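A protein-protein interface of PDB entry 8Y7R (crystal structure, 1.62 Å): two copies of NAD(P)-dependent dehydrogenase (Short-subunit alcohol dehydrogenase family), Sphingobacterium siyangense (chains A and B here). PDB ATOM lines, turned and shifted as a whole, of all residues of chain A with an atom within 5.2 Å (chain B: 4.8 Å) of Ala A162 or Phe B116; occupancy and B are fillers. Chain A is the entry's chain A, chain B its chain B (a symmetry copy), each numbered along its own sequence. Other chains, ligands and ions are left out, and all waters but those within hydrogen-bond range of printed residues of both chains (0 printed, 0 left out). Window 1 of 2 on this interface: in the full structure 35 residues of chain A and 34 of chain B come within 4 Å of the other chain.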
ATOM      1  N   TRP A 108     -20.170  22.806  11.334  1.00  0.00           N
ATOM      2  CA  TRP A 108     -20.799  21.512  11.026  1.00  0.00           C
ATOM      3  C   TRP A 108     -21.397  20.852  12.271  1.00  0.00           C
ATOM      4  O   TRP A 108     -22.576  20.489  12.328  1.00  0.00           O
ATOM      5  CB  TRP A 108     -19.782  20.588  10.404  1.00  0.00           C
ATOM      6  CG  TRP A 108     -20.335  19.229  10.085  1.00  0.00           C
ATOM      7  CD1 TRP A 108     -20.247  18.149  10.897  1.00  0.00           C
ATOM      8  CD2 TRP A 108     -21.009  18.797   8.875  1.00  0.00           C
ATOM      9  NE1 TRP A 108     -20.895  17.094  10.336  1.00  0.00           N
ATOM     10  CE2 TRP A 108     -21.353  17.452   9.101  1.00  0.00           C
ATOM     11  CE3 TRP A 108     -21.340  19.399   7.660  1.00  0.00           C
ATOM     12  CZ2 TRP A 108     -22.050  16.699   8.146  1.00  0.00           C
ATOM     13  CZ3 TRP A 108     -22.013  18.651   6.707  1.00  0.00           C
ATOM     14  CH2 TRP A 108     -22.366  17.335   6.982  1.00  0.00           C
ATOM     15  N   ILE A 112     -25.260  19.831  13.219  1.00  0.00           N
ATOM     16  CA  ILE A 112     -25.610  18.427  13.403  1.00  0.00           C
ATOM     17  C   ILE A 112     -26.148  18.194  14.826  1.00  0.00           C
ATOM     18  O   ILE A 112     -27.153  17.504  15.074  1.00  0.00           O
ATOM     19  CB  ILE A 112     -24.451  17.498  13.051  1.00  0.00           C
ATOM     20  CG1 ILE A 112     -23.966  17.604  11.599  1.00  0.00           C
ATOM     21  CG2 ILE A 112     -24.759  16.041  13.434  1.00  0.00           C
ATOM     22  CD1 ILE A 112     -24.990  17.954  10.561  1.00  0.00           C
ATOM     23  N   PHE A 116     -30.088  17.557  14.397  1.00  0.00           N
ATOM     24  CA  PHE A 116     -30.226  16.139  14.254  1.00  0.00           C
ATOM     25  C   PHE A 116     -30.046  15.413  15.585  1.00  0.00           C
ATOM     26  O   PHE A 116     -31.010  14.809  16.054  1.00  0.00           O
ATOM     27  CB  PHE A 116     -29.319  15.577  13.186  1.00  0.00           C
ATOM     28  CG  PHE A 116     -29.420  14.065  13.217  1.00  0.00           C
ATOM     29  CD1 PHE A 116     -30.657  13.426  13.131  1.00  0.00           C
ATOM     30  CD2 PHE A 116     -28.306  13.327  13.480  1.00  0.00           C
ATOM     31  CE1 PHE A 116     -30.721  12.043  13.252  1.00  0.00           C
ATOM     32  CE2 PHE A 116     -28.360  11.951  13.514  1.00  0.00           C
ATOM     33  CZ  PHE A 116     -29.565  11.325  13.464  1.00  0.00           C
ATOM     34  N   THR A 157     -28.824  20.332   5.282  1.00  0.00           N
ATOM     35  CA  THR A 157     -29.405  19.314   4.399  1.00  0.00           C
ATOM     36  C   THR A 157     -29.169  17.919   4.955  1.00  0.00           C
ATOM     37  O   THR A 157     -30.076  17.080   5.015  1.00  0.00           O
ATOM     38  CB  THR A 157     -28.835  19.457   3.002  1.00  0.00           C
ATOM     39  OG1 THR A 157     -29.137  20.745   2.486  1.00  0.00           O
ATOM     40  CG2 THR A 157     -29.391  18.430   2.016  1.00  0.00           C
ATOM     41  N   SER A 158     -27.930  17.642   5.383  1.00  0.00           N
ATOM     42  CA  SER A 158     -27.605  16.328   5.904  1.00  0.00           C
ATOM     43  C   SER A 158     -28.414  16.029   7.173  1.00  0.00           C
ATOM     44  O   SER A 158     -29.011  14.952   7.345  1.00  0.00           O
ATOM     45  CB  SER A 158     -26.109  16.240   6.180  1.00  0.00           C
ATOM     46  OG  SER A 158     -25.351  16.471   4.999  1.00  0.00           O
ATOM     47  N   ALA A 159     -28.469  17.007   8.094  1.00  0.00           N
ATOM     48  CA  ALA A 159     -29.229  16.864   9.315  1.00  0.00           C
ATOM     49  C   ALA A 159     -30.709  16.625   9.031  1.00  0.00           C
ATOM     50  O   ALA A 159     -31.330  15.787   9.695  1.00  0.00           O
ATOM     51  CB  ALA A 159     -29.049  18.046  10.215  1.00  0.00           C
ATOM     52  N   LYS A 160     -31.308  17.389   8.097  1.00  0.00           N
ATOM     53  CA  LYS A 160     -32.739  17.248   7.842  1.00  0.00           C
ATOM     54  C   LYS A 160     -33.054  15.910   7.158  1.00  0.00           C
ATOM     55  O   LYS A 160     -34.076  15.313   7.457  1.00  0.00           O
ATOM     56  CB  LYS A 160     -33.268  18.454   7.067  1.00  0.00           C
ATOM     57  CG  LYS A 160     -33.131  19.752   7.847  1.00  0.00           C
ATOM     58  CD  LYS A 160     -33.990  19.752   9.102  1.00  0.00           C
ATOM     59  CE  LYS A 160     -34.209  21.097   9.760  1.00  0.00           C
ATOM     60  NZ  LYS A 160     -35.101  20.986  10.936  1.00  0.00           N
ATOM     61  N   HIS A 161     -32.174  15.431   6.264  1.00  0.00           N
ATOM     62  CA  HIS A 161     -32.254  14.068   5.755  1.00  0.00           C
ATOM     63  C   HIS A 161     -32.271  13.075   6.911  1.00  0.00           C
ATOM     64  O   HIS A 161     -33.056  12.115   6.946  1.00  0.00           O
ATOM     65  CB  HIS A 161     -31.139  13.725   4.758  1.00  0.00           C
ATOM     66  CG  HIS A 161     -31.432  14.131   3.353  1.00  0.00           C
ATOM     67  ND1 HIS A 161     -31.469  15.447   2.953  1.00  0.00           N
ATOM     68  CD2 HIS A 161     -31.547  13.370   2.221  1.00  0.00           C
ATOM     69  CE1 HIS A 161     -31.784  15.454   1.630  1.00  0.00           C
ATOM     70  NE2 HIS A 161     -31.810  14.189   1.174  1.00  0.00           N
ATOM     71  N   ALA A 162     -31.320  13.229   7.846  1.00  0.00           N
ATOM     72  CA  ALA A 162     -31.236  12.340   9.003  1.00  0.00           C
ATOM     73  C   ALA A 162     -32.508  12.316   9.827  1.00  0.00           C
ATOM     74  O   ALA A 162     -32.943  11.239  10.258  1.00  0.00           O
ATOM     75  CB  ALA A 162     -30.069  12.785   9.837  1.00  0.00           C
ATOM     76  N   VAL A 163     -33.154  13.486  10.018  1.00  0.00           N
ATOM     77  CA  VAL A 163     -34.426  13.533  10.719  1.00  0.00           C
ATOM     78  C   VAL A 163     -35.492  12.709  10.013  1.00  0.00           C
ATOM     79  O   VAL A 163     -36.299  12.029  10.660  1.00  0.00           O
ATOM     80  CB  VAL A 163     -34.906  14.987  10.881  1.00  0.00           C
ATOM     81  CG1 VAL A 163     -36.338  15.091  11.357  1.00  0.00           C
ATOM     82  CG2 VAL A 163     -34.004  15.824  11.777  1.00  0.00           C
ATOM     83  N   VAL A 164     -35.532  12.758   8.655  1.00  0.00           N
ATOM     84  CA  VAL A 164     -36.464  11.910   7.924  1.00  0.00           C
ATOM     85  C   VAL A 164     -36.209  10.426   8.217  1.00  0.00           C
ATOM     86  O   VAL A 164     -37.154   9.683   8.471  1.00  0.00           O
ATOM     87  CB  VAL A 164     -36.402  12.209   6.412  1.00  0.00           C
ATOM     88  CG1 VAL A 164     -37.235  11.228   5.602  1.00  0.00           C
ATOM     89  CG2 VAL A 164     -36.795  13.658   6.143  1.00  0.00           C
ATOM     90  N   GLY A 165     -34.947   9.981   8.193  1.00  0.00           N
ATOM     91  CA  GLY A 165     -34.613   8.577   8.461  1.00  0.00           C
ATOM     92  C   GLY A 165     -34.997   8.147   9.898  1.00  0.00           C
ATOM     93  O   GLY A 165     -35.587   7.074  10.092  1.00  0.00           O
ATOM     94  N   LEU A 166     -34.707   9.028  10.871  1.00  0.00           N
ATOM     95  CA  LEU A 166     -35.066   8.761  12.259  1.00  0.00           C
ATOM     96  C   LEU A 166     -36.574   8.575  12.386  1.00  0.00           C
ATOM     97  O   LEU A 166     -37.060   7.674  13.080  1.00  0.00           O
ATOM     98  CB  LEU A 166     -34.563   9.898  13.140  1.00  0.00           C
ATOM     99  CG  LEU A 166     -35.005   9.849  14.605  1.00  0.00           C
ATOM    100  CD1 LEU A 166     -34.450   8.612  15.262  1.00  0.00           C
ATOM    101  CD2 LEU A 166     -34.618  11.129  15.325  1.00  0.00           C
ATOM    102  N   THR A 167     -37.321   9.438  11.685  1.00  0.00           N
ATOM    103  CA  THR A 167     -38.770   9.402  11.689  1.00  0.00           C
ATOM    104  C   THR A 167     -39.288   8.054  11.181  1.00  0.00           C
ATOM    105  O   THR A 167     -40.224   7.491  11.746  1.00  0.00           O
ATOM    106  CB  THR A 167     -39.324  10.590  10.897  1.00  0.00           C
ATOM    107  OG1 THR A 167     -38.900  11.821  11.514  1.00  0.00           O
ATOM    108  CG2 THR A 167     -40.830  10.578  10.801  1.00  0.00           C
ATOM    109  N   VAL B 111     -22.098   5.730  16.338  1.00  0.00           N
ATOM    110  CA  VAL B 111     -22.623   5.431  15.003  1.00  0.00           C
ATOM    111  C   VAL B 111     -22.698   6.727  14.191  1.00  0.00           C
ATOM    112  O   VAL B 111     -22.270   6.774  13.021  1.00  0.00           O
ATOM    113  CB  VAL B 111     -23.995   4.721  15.053  1.00  0.00           C
ATOM    114  CG1 VAL B 111     -24.618   4.661  13.660  1.00  0.00           C
ATOM    115  CG2 VAL B 111     -23.924   3.327  15.672  1.00  0.00           C
ATOM    116  N   ILE B 112     -23.210   7.798  14.780  1.00  0.00           N
ATOM    117  CA  ILE B 112     -23.321   9.058  14.043  1.00  0.00           C
ATOM    118  C   ILE B 112     -21.931   9.617  13.699  1.00  0.00           C
ATOM    119  O   ILE B 112     -21.651  10.104  12.598  1.00  0.00           O
ATOM    120  CB  ILE B 112     -24.148  10.075  14.852  1.00  0.00           C
ATOM    121  CG1 ILE B 112     -25.576   9.547  15.125  1.00  0.00           C
ATOM    122  CG2 ILE B 112     -24.177  11.463  14.214  1.00  0.00           C
ATOM    123  CD1 ILE B 112     -26.294   8.970  13.918  1.00  0.00           C
ATOM    124  N   ASP B 113     -21.000   9.515  14.647  1.00  0.00           N
ATOM    125  CA  ASP B 113     -19.669  10.049  14.382  1.00  0.00           C
ATOM    126  C   ASP B 113     -18.982   9.338  13.248  1.00  0.00           C
ATOM    127  O   ASP B 113     -18.278  10.025  12.486  1.00  0.00           O
ATOM    128  CB  ASP B 113     -18.794  10.107  15.632  1.00  0.00           C
ATOM    129  CG  ASP B 113     -19.143  11.196  16.633  1.00  0.00           C
ATOM    130  OD1 ASP B 113     -19.940  12.144  16.290  1.00  0.00           O
ATOM    131  OD2 ASP B 113     -18.642  11.092  17.794  1.00  0.00           O
ATOM    132  N   ILE B 114     -19.106   8.014  13.140  1.00  0.00           N
ATOM    133  CA  ILE B 114     -18.438   7.245  12.113  1.00  0.00           C
ATOM    134  C   ILE B 114     -19.214   7.378  10.802  1.00  0.00           C
ATOM    135  O   ILE B 114     -18.630   7.775   9.795  1.00  0.00           O
ATOM    136  CB  ILE B 114     -18.238   5.769  12.515  1.00  0.00           C
ATOM    137  CG1 ILE B 114     -17.257   5.685  13.702  1.00  0.00           C
ATOM    138  CG2 ILE B 114     -17.756   4.884  11.366  1.00  0.00           C
ATOM    139  CD1 ILE B 114     -17.292   4.348  14.408  1.00  0.00           C
ATOM    140  N   ASN B 115     -20.530   7.083  10.861  1.00  0.00           N
ATOM    141  CA  ASN B 115     -21.299   6.868   9.643  1.00  0.00           C
ATOM    142  C   ASN B 115     -21.789   8.170   8.999  1.00  0.00           C
ATOM    143  O   ASN B 115     -22.200   8.092   7.838  1.00  0.00           O
ATOM    144  CB  ASN B 115     -22.490   5.981   9.914  1.00  0.00           C
ATOM    145  CG  ASN B 115     -22.065   4.592  10.299  1.00  0.00           C
ATOM    146  OD1 ASN B 115     -20.886   4.352  10.585  1.00  0.00           O
ATOM    147  ND2 ASN B 115     -23.004   3.680  10.295  1.00  0.00           N
ATOM    148  N   PHE B 116     -21.874   9.269   9.756  1.00  0.00           N
ATOM    149  CA  PHE B 116     -22.420  10.554   9.313  1.00  0.00           C
ATOM    150  C   PHE B 116     -21.247  11.540   9.266  1.00  0.00           C
ATOM    151  O   PHE B 116     -20.753  11.945   8.218  1.00  0.00           O
ATOM    152  CB  PHE B 116     -23.552  10.963  10.279  1.00  0.00           C
ATOM    153  CG  PHE B 116     -24.394  12.239  10.102  1.00  0.00           C
ATOM    154  CD1 PHE B 116     -23.900  13.308   9.425  1.00  0.00           C
ATOM    155  CD2 PHE B 116     -25.684  12.335  10.666  1.00  0.00           C
ATOM    156  CE1 PHE B 116     -24.666  14.430   9.203  1.00  0.00           C
ATOM    157  CE2 PHE B 116     -26.433  13.488  10.529  1.00  0.00           C
ATOM    158  CZ  PHE B 116     -25.928  14.541   9.793  1.00  0.00           C
ATOM    159  N   ASN B 117     -20.780  11.934  10.443  1.00  0.00           N
ATOM    160  CA  ASN B 117     -19.790  12.998  10.507  1.00  0.00           C
ATOM    161  C   ASN B 117     -18.526  12.603   9.747  1.00  0.00           C
ATOM    162  O   ASN B 117     -17.931  13.436   9.037  1.00  0.00           O
ATOM    163  CB  ASN B 117     -19.496  13.378  11.961  1.00  0.00           C
ATOM    164  CG  ASN B 117     -20.637  14.106  12.643  1.00  0.00           C
ATOM    165  OD1 ASN B 117     -21.406  14.860  12.019  1.00  0.00           O
ATOM    166  ND2 ASN B 117     -20.821  13.793  13.923  1.00  0.00           N
ATOM    167  N   GLY B 118     -18.101  11.342   9.870  1.00  0.00           N
ATOM    168  CA  GLY B 118     -16.854  10.900   9.274  1.00  0.00           C
ATOM    169  C   GLY B 118     -16.893  10.938   7.751  1.00  0.00           C
ATOM    170  O   GLY B 118     -15.904  11.259   7.091  1.00  0.00           O
ATOM    171  N   VAL B 119     -18.099  10.770   7.160  1.00  0.00           N
ATOM    172  CA  VAL B 119     -18.203  10.847   5.724  1.00  0.00           C
ATOM    173  C   VAL B 119     -18.017  12.305   5.291  1.00  0.00           C
ATOM    174  O   VAL B 119     -17.433  12.588   4.239  1.00  0.00           O
ATOM    175  CB  VAL B 119     -19.553  10.246   5.260  1.00  0.00           C
ATOM    176  CG1 VAL B 119     -19.733  10.471   3.768  1.00  0.00           C
ATOM    177  CG2 VAL B 119     -19.622   8.785   5.638  1.00  0.00           C
ATOM    178  N   PHE B 120     -18.597  13.233   6.052  1.00  0.00           N
ATOM    179  CA  PHE B 120     -18.394  14.626   5.792  1.00  0.00           C
ATOM    180  C   PHE B 120     -16.889  14.979   5.905  1.00  0.00           C
ATOM    181  O   PHE B 120     -16.385  15.714   5.068  1.00  0.00           O
ATOM    182  CB  PHE B 120     -19.231  15.549   6.678  1.00  0.00           C
ATOM    183  CG  PHE B 120     -18.681  16.972   6.759  1.00  0.00           C
ATOM    184  CD1 PHE B 120     -18.756  17.832   5.673  1.00  0.00           C
ATOM    185  CD2 PHE B 120     -18.051  17.420   7.922  1.00  0.00           C
ATOM    186  CE1 PHE B 120     -18.174  19.098   5.709  1.00  0.00           C
ATOM    187  CE2 PHE B 120     -17.551  18.718   7.988  1.00  0.00           C
ATOM    188  CZ  PHE B 120     -17.611  19.536   6.906  1.00  0.00           C
ATOM    189  N   SER B 158     -30.487   6.855  10.247  1.00  0.00           N
ATOM    190  CA  SER B 158     -30.408   8.310  10.256  1.00  0.00           C
ATOM    191  C   SER B 158     -29.128   8.748   9.537  1.00  0.00           C
ATOM    192  O   SER B 158     -29.128   9.669   8.711  1.00  0.00           O
ATOM    193  CB  SER B 158     -30.441   8.834  11.665  1.00  0.00           C
ATOM    194  OG  SER B 158     -31.648   8.498  12.302  1.00  0.00           O
ATOM    195  N   ALA B 159     -27.992   8.079   9.872  1.00  0.00           N
ATOM    196  CA  ALA B 159     -26.718   8.435   9.272  1.00  0.00           C
ATOM    197  C   ALA B 159     -26.720   8.184   7.773  1.00  0.00           C
ATOM    198  O   ALA B 159     -26.151   8.976   7.022  1.00  0.00           O
ATOM    199  CB  ALA B 159     -25.580   7.659   9.939  1.00  0.00           C
ATOM    200  N   HIS B 161     -29.318   8.136   5.704  1.00  0.00           N
ATOM    201  CA  HIS B 161     -30.102   9.245   5.118  1.00  0.00           C
ATOM    202  C   HIS B 161     -29.263  10.529   4.985  1.00  0.00           C
ATOM    203  O   HIS B 161     -29.244  11.195   3.952  1.00  0.00           O
ATOM    204  CB  HIS B 161     -31.353   9.535   5.929  1.00  0.00           C
ATOM    205  CG  HIS B 161     -32.545   8.663   5.619  1.00  0.00           C
ATOM    206  ND1 HIS B 161     -32.560   7.304   5.867  1.00  0.00           N
ATOM    207  CD2 HIS B 161     -33.764   9.001   5.173  1.00  0.00           C
ATOM    208  CE1 HIS B 161     -33.750   6.845   5.438  1.00  0.00           C
ATOM    209  NE2 HIS B 161     -34.485   7.850   5.048  1.00  0.00           N
ATOM    210  N   ALA B 162     -28.502  10.872   6.050  1.00  0.00           N
ATOM    211  CA  ALA B 162     -27.640  12.036   6.002  1.00  0.00           C
ATOM    212  C   ALA B 162     -26.655  11.956   4.859  1.00  0.00           C
ATOM    213  O   ALA B 162     -26.396  12.978   4.198  1.00  0.00           O
ATOM    214  CB  ALA B 162     -26.890  12.180   7.350  1.00  0.00           C
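Of the 14 printed residues of chain B, 7 touch a printed residue of chain A. Printed residues of chain B that touch a printed residue of chain A: Ile B112, Phe B116, Asn B117, Phe B120, Ser B158, His B161 and Ala B162. Hydrophobic or aromatic side chains of chain B within 4 Å of the printed part of chain A: Ile B112, Phe B116, Phe B120, His B161 and Ala B162. Along chain B the printed residues that touch a printed residue of chain A span positions 112 to 162. Printed residues of chain A that touch a printed residue of chain B: Trp A108, Ile A112, Phe A116, Ser A158, Ala A159, His A161, Ala A162, Gly A165 and Leu A166. Hydrophobic or aromatic side chains of chain A that line the printed part of chain B: Trp A108, Ile A112, Phe A116, His A161, Ala A162 and Leu A166. Among the printed residues, 16 pairs touch across the chains. Among the printed residues, no Asp or Glu carboxylate lies within 4 Å of a Lys or Arg side-chain nitrogen of the other chain.
Of the printed residues of chain B, Ala A162 touches Phe B116 and Ser B158. Of chain A, only Trp A108 (3.6 Å), Ile A112 (3.6 Å), Phe A116 (3.5 Å), Ser A158 (3.8 Å), Ala A159 (3.9 Å) and Ala A162 (3.8 Å) come within 4 Å of Phe B116. Of the printed residues of chain A, His B161 touches His A161 (3.3 Å) and Gly A165 (3.4 Å). Of the printed residues of chain A, Phe B120 touches Trp A108 (3.4 Å). The nearest printed residue of chain A that does not touch Phe B116 is Lys A160 (6.3 Å). The nearest printed residue of chain B that does not touch Phe A116 is Ala B159 (5.1 Å).
The side-chain amide oxygen (OD1) of Asn B117 sits at hydrogen-bond distance from the indole nitrogen (NE1) of Trp A108, 2.8 Å away. The side-chain hydroxyl of Ser B158 lies close to the backbone NH of Leu A166.
Ile A112 touches Phe B116, and with the chains exchanged Phe A116 touches Ile B112. Phe B116 touches its own counterpart, Phe A116. Ser A158 touches Ala B162, and with the chains exchanged Ala A162 touches Ser B158. Ala A159 touches Phe B116, but with the chains exchanged Phe A116 does not touch Ala B159 (5.1 Å). Of the 16 pairs that touch across the chains among the printed residues, 8 have their exchanged pair printed and touching as well.
Among the printed residues, pairs that only touch across the chains: Trp A108 with Phe B116 (3.6 Å), Trp A108 with Phe B120 (3.4 Å), Ile A112 with Phe B116 (3.6 Å), Ile A112 with Asn B117 (3.8 Å), Phe A116 with Ile B112 (3.6 Å), Phe A116 with Phe B116 (3.5 Å), Phe A116 with Ser B158 (3.2 Å), Ser A158 with Phe B116 (3.8 Å), Ser A158 with Ala B162 (3.5 Å), Ala A159 with Phe B116 (3.9 Å), His A161 with His B161 (3.3 Å), Ala A162 with Phe B116 (3.8 Å), Ala A162 with Ser B158 (3.4 Å) and Gly A165 with His B161 (3.4 Å).
The side-chain amide nitrogen (ND2) of Asn B117 is in hydrogen-bond range of the side-chain carboxylate (OD1) of Asp B113 (3.0 Å). The backbone carbonyl oxygen (O) of Thr A157 sits at hydrogen-bond distance from a ring nitrogen (ND1) of His A161 (3.0 Å). The backbone carbonyl oxygen of Ile B112 lies within hydrogen-bond range of the backbone NH of Asn B117, at 3.0 Å.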
